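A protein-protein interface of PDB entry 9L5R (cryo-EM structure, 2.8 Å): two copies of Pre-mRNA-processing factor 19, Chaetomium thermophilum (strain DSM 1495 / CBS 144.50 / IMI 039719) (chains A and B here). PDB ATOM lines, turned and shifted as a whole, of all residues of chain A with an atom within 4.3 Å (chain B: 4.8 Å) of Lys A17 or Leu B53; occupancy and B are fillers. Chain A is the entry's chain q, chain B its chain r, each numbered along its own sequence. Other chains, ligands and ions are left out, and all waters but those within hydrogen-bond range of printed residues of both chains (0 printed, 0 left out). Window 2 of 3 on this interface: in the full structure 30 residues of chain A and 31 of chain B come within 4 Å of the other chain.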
ATOM      1  N   VAL A  15      11.278 -10.556 -17.886  1.00  0.00           N
ATOM      2  CA  VAL A  15      10.996 -11.209 -16.614  1.00  0.00           C
ATOM      3  C   VAL A  15      12.028 -12.301 -16.377  1.00  0.00           C
ATOM      4  O   VAL A  15      12.246 -13.159 -17.241  1.00  0.00           O
ATOM      5  CB  VAL A  15       9.573 -11.793 -16.594  1.00  0.00           C
ATOM      6  CG1 VAL A  15       9.347 -12.629 -15.342  1.00  0.00           C
ATOM      7  CG2 VAL A  15       8.552 -10.685 -16.688  1.00  0.00           C
ATOM      8  N   SER A  16      12.663 -12.265 -15.208  1.00  0.00           N
ATOM      9  CA  SER A  16      13.475 -13.385 -14.753  1.00  0.00           C
ATOM     10  C   SER A  16      12.572 -14.578 -14.471  1.00  0.00           C
ATOM     11  O   SER A  16      11.647 -14.483 -13.660  1.00  0.00           O
ATOM     12  CB  SER A  16      14.255 -12.994 -13.501  1.00  0.00           C
ATOM     13  OG  SER A  16      14.873 -14.124 -12.913  1.00  0.00           O
ATOM     14  N   LYS A  17      12.834 -15.703 -15.139  1.00  0.00           N
ATOM     15  CA  LYS A  17      11.981 -16.874 -14.965  1.00  0.00           C
ATOM     16  C   LYS A  17      12.189 -17.545 -13.615  1.00  0.00           C
ATOM     17  O   LYS A  17      11.272 -18.203 -13.109  1.00  0.00           O
ATOM     18  CB  LYS A  17      12.230 -17.886 -16.083  1.00  0.00           C
ATOM     19  CG  LYS A  17      11.631 -17.502 -17.423  1.00  0.00           C
ATOM     20  CD  LYS A  17      11.907 -18.578 -18.456  1.00  0.00           C
ATOM     21  CE  LYS A  17      11.376 -18.191 -19.822  1.00  0.00           C
ATOM     22  NZ  LYS A  17      11.949 -19.042 -20.899  1.00  0.00           N
ATOM     23  N   LYS A  18      13.375 -17.399 -13.023  1.00  0.00           N
ATOM     24  CA  LYS A  18      13.672 -18.116 -11.789  1.00  0.00           C
ATOM     25  C   LYS A  18      12.957 -17.499 -10.591  1.00  0.00           C
ATOM     26  O   LYS A  18      12.458 -18.224  -9.722  1.00  0.00           O
ATOM     27  CB  LYS A  18      15.182 -18.154 -11.561  1.00  0.00           C
ATOM     28  CG  LYS A  18      15.950 -18.865 -12.665  1.00  0.00           C
ATOM     29  CD  LYS A  18      15.495 -20.307 -12.810  1.00  0.00           C
ATOM     30  CE  LYS A  18      15.876 -21.127 -11.591  1.00  0.00           C
ATOM     31  NZ  LYS A  18      17.351 -21.208 -11.430  1.00  0.00           N
ATOM     32  N   THR A  19      12.887 -16.170 -10.528  1.00  0.00           N
ATOM     33  CA  THR A  19      12.322 -15.491  -9.373  1.00  0.00           C
ATOM     34  C   THR A  19      11.112 -14.621  -9.683  1.00  0.00           C
ATOM     35  O   THR A  19      10.417 -14.214  -8.746  1.00  0.00           O
ATOM     36  CB  THR A  19      13.387 -14.621  -8.690  1.00  0.00           C
ATOM     37  OG1 THR A  19      14.009 -13.781  -9.668  1.00  0.00           O
ATOM     38  CG2 THR A  19      14.447 -15.487  -8.034  1.00  0.00           C
ATOM     39  N   THR A  50      17.632 -18.461 -21.860  1.00  0.00           N
ATOM     40  CA  THR A  50      16.636 -19.422 -21.398  1.00  0.00           C
ATOM     41  C   THR A  50      15.859 -18.953 -20.179  1.00  0.00           C
ATOM     42  O   THR A  50      14.652 -19.188 -20.103  1.00  0.00           O
ATOM     43  CB  THR A  50      17.280 -20.786 -21.077  1.00  0.00           C
ATOM     44  OG1 THR A  50      17.915 -20.732 -19.795  1.00  0.00           O
ATOM     45  CG2 THR A  50      18.301 -21.182 -22.134  1.00  0.00           C
ATOM     46  N   ASP A  51      16.511 -18.300 -19.218  1.00  0.00           N
ATOM     47  CA  ASP A  51      15.849 -17.913 -17.978  1.00  0.00           C
ATOM     48  C   ASP A  51      15.308 -16.488 -17.995  1.00  0.00           C
ATOM     49  O   ASP A  51      14.781 -16.035 -16.973  1.00  0.00           O
ATOM     50  CB  ASP A  51      16.801 -18.077 -16.790  1.00  0.00           C
ATOM     51  CG  ASP A  51      16.937 -19.518 -16.348  1.00  0.00           C
ATOM     52  OD1 ASP A  51      16.045 -20.328 -16.676  1.00  0.00           O
ATOM     53  OD2 ASP A  51      17.936 -19.841 -15.670  1.00  0.00           O
ATOM     54  N   LEU A  52      15.428 -15.769 -19.105  1.00  0.00           N
ATOM     55  CA  LEU A  52      14.826 -14.447 -19.233  1.00  0.00           C
ATOM     56  C   LEU A  52      13.724 -14.467 -20.283  1.00  0.00           C
ATOM     57  O   LEU A  52      13.839 -15.148 -21.307  1.00  0.00           O
ATOM     58  CB  LEU A  52      15.868 -13.381 -19.584  1.00  0.00           C
ATOM     59  CG  LEU A  52      16.600 -12.705 -18.414  1.00  0.00           C
ATOM     60  CD1 LEU A  52      15.594 -12.002 -17.514  1.00  0.00           C
ATOM     61  CD2 LEU A  52      17.482 -13.644 -17.605  1.00  0.00           C
ATOM     62  N   LEU A  53      12.653 -13.716 -20.018  1.00  0.00           N
ATOM     63  CA  LEU A  53      11.467 -13.701 -20.867  1.00  0.00           C
ATOM     64  C   LEU A  53      10.853 -12.309 -20.933  1.00  0.00           C
ATOM     65  O   LEU A  53      10.577 -11.704 -19.891  1.00  0.00           O
ATOM     66  CB  LEU A  53      10.428 -14.690 -20.344  1.00  0.00           C
ATOM     67  CG  LEU A  53       9.051 -14.622 -21.003  1.00  0.00           C
ATOM     68  CD1 LEU A  53       9.076 -15.221 -22.400  1.00  0.00           C
ATOM     69  CD2 LEU A  53       8.019 -15.307 -20.133  1.00  0.00           C
ATOM     70  N   VAL B  14       0.393 -11.594 -12.934  1.00  0.00           N
ATOM     71  CA  VAL B  14       0.988 -12.892 -13.236  1.00  0.00           C
ATOM     72  C   VAL B  14       1.247 -12.977 -14.733  1.00  0.00           C
ATOM     73  O   VAL B  14       0.357 -12.691 -15.542  1.00  0.00           O
ATOM     74  CB  VAL B  14       0.084 -14.055 -12.771  1.00  0.00           C
ATOM     75  CG1 VAL B  14       0.685 -15.396 -13.158  1.00  0.00           C
ATOM     76  CG2 VAL B  14      -0.134 -13.999 -11.267  1.00  0.00           C
ATOM     77  N   VAL B  15       2.460 -13.373 -15.106  1.00  0.00           N
ATOM     78  CA  VAL B  15       2.846 -13.493 -16.508  1.00  0.00           C
ATOM     79  C   VAL B  15       2.574 -14.918 -16.966  1.00  0.00           C
ATOM     80  O   VAL B  15       3.164 -15.871 -16.444  1.00  0.00           O
ATOM     81  CB  VAL B  15       4.324 -13.134 -16.721  1.00  0.00           C
ATOM     82  CG1 VAL B  15       4.749 -13.472 -18.144  1.00  0.00           C
ATOM     83  CG2 VAL B  15       4.576 -11.669 -16.423  1.00  0.00           C
ATOM     84  N   LYS B  17       3.685 -17.390 -19.280  1.00  0.00           N
ATOM     85  CA  LYS B  17       5.014 -17.444 -19.876  1.00  0.00           C
ATOM     86  C   LYS B  17       5.032 -18.084 -21.257  1.00  0.00           C
ATOM     87  O   LYS B  17       5.978 -17.844 -22.016  1.00  0.00           O
ATOM     88  CB  LYS B  17       5.980 -18.194 -18.954  1.00  0.00           C
ATOM     89  CG  LYS B  17       5.721 -19.685 -18.837  1.00  0.00           C
ATOM     90  CD  LYS B  17       6.839 -20.377 -18.078  1.00  0.00           C
ATOM     91  CE  LYS B  17       6.935 -19.863 -16.652  1.00  0.00           C
ATOM     92  NZ  LYS B  17       5.719 -20.192 -15.859  1.00  0.00           N
ATOM     93  N   ASP B  51       2.715 -23.189 -15.740  1.00  0.00           N
ATOM     94  CA  ASP B  51       2.949 -22.228 -16.811  1.00  0.00           C
ATOM     95  C   ASP B  51       2.589 -20.800 -16.422  1.00  0.00           C
ATOM     96  O   ASP B  51       2.948 -19.872 -17.152  1.00  0.00           O
ATOM     97  CB  ASP B  51       2.169 -22.631 -18.063  1.00  0.00           C
ATOM     98  CG  ASP B  51       2.702 -23.900 -18.698  1.00  0.00           C
ATOM     99  OD1 ASP B  51       3.895 -24.211 -18.498  1.00  0.00           O
ATOM    100  OD2 ASP B  51       1.928 -24.588 -19.395  1.00  0.00           O
ATOM    101  N   LEU B  52       1.888 -20.598 -15.311  1.00  0.00           N
ATOM    102  CA  LEU B  52       1.660 -19.249 -14.813  1.00  0.00           C
ATOM    103  C   LEU B  52       2.811 -18.818 -13.912  1.00  0.00           C
ATOM    104  O   LEU B  52       3.160 -19.518 -12.957  1.00  0.00           O
ATOM    105  CB  LEU B  52       0.336 -19.175 -14.056  1.00  0.00           C
ATOM    106  CG  LEU B  52      -0.885 -18.903 -14.931  1.00  0.00           C
ATOM    107  CD1 LEU B  52      -2.095 -18.666 -14.060  1.00  0.00           C
ATOM    108  CD2 LEU B  52      -0.639 -17.712 -15.848  1.00  0.00           C
ATOM    109  N   LEU B  53       3.399 -17.668 -14.220  1.00  0.00           N
ATOM    110  CA  LEU B  53       4.532 -17.137 -13.461  1.00  0.00           C
ATOM    111  C   LEU B  53       4.213 -15.740 -12.952  1.00  0.00           C
ATOM    112  O   LEU B  53       4.111 -14.798 -13.761  1.00  0.00           O
ATOM    113  CB  LEU B  53       5.793 -17.114 -14.325  1.00  0.00           C
ATOM    114  CG  LEU B  53       7.074 -16.654 -13.628  1.00  0.00           C
ATOM    115  CD1 LEU B  53       7.479 -17.641 -12.545  1.00  0.00           C
ATOM    116  CD2 LEU B  53       8.197 -16.473 -14.638  1.00  0.00           C
ATOM    117  N   PRO B  54       4.045 -15.547 -11.646  1.00  0.00           N
ATOM    118  CA  PRO B  54       3.740 -14.210 -11.130  1.00  0.00           C
ATOM    119  C   PRO B  54       4.956 -13.299 -11.165  1.00  0.00           C
ATOM    120  O   PRO B  54       6.103 -13.740 -11.260  1.00  0.00           O
ATOM    121  CB  PRO B  54       3.294 -14.481  -9.691  1.00  0.00           C
ATOM    122  CG  PRO B  54       4.013 -15.732  -9.318  1.00  0.00           C
ATOM    123  CD  PRO B  54       4.107 -16.556 -10.575  1.00  0.00           C
ATOM    124  N   ILE B  55       4.685 -11.998 -11.087  1.00  0.00           N
ATOM    125  CA  ILE B  55       5.729 -10.983 -11.025  1.00  0.00           C
ATOM    126  C   ILE B  55       5.719 -10.380  -9.624  1.00  0.00           C
ATOM    127  O   ILE B  55       4.706 -10.421  -8.914  1.00  0.00           O
ATOM    128  CB  ILE B  55       5.547  -9.904 -12.121  1.00  0.00           C
ATOM    129  CG1 ILE B  55       6.856  -9.156 -12.388  1.00  0.00           C
ATOM    130  CG2 ILE B  55       4.465  -8.913 -11.744  1.00  0.00           C
ATOM    131  CD1 ILE B  55       7.901  -9.983 -13.092  1.00  0.00           C
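The backbone NH (N) of Lys A17 is in hydrogen-bond range of the backbone carbonyl oxygen (O) of Asp A51. The backbone carbonyl oxygen (O) of Leu B53 sits at hydrogen-bond distance from the backbone NH (N) of Val B15, at 2.6 Å. The backbone carbonyl oxygen (O) of Thr A50 sits at hydrogen-bond distance from the side-chain amino group (NZ) of Lys A17. N of Val A15 lies within hydrogen-bond range of O of Leu A53, 2.4 Å away. NZ of Lys B17 sits at hydrogen-bond distance from O of Asp B51 (3.1 Å).
Printed residues of chain B within 4 Å of Val A15: Ile B55 (3.7 Å). Of the printed residues of chain A, Lys B17 touches Leu A53. Printed residues of chain A within 4 Å of Ile B55: Val A15. Thr A19 touches none of the printed residues of chain B. The nearest printed residue of chain B that does not touch Lys A17 is Lys B17 (5.3 Å). The nearest printed residue of chain A that does not touch Leu B53 is Val A15 (4.1 Å). The nearest printed residue of chain B that does not touch Val A15 is Leu B53 (4.1 Å).
Lys A17 touches Leu B53, and with the chains exchanged Leu A53 touches Lys B17. 5 positions are printed for both chains.
Among the printed residues, merely in contact across the chains: Val A15 with Ile B55 (3.7 Å), Lys A17 with Leu B53 (3.8 Å) and Leu A53 with Lys B17 (3.7 Å).
Of the 9 printed residues of chain A, 3 touch a printed residue of chain B. Of the 8 printed residues of chain B, 3 touch a printed residue of chain A. Along chain B the printed residues that touch a printed residue of chain A span positions 17 to 55.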
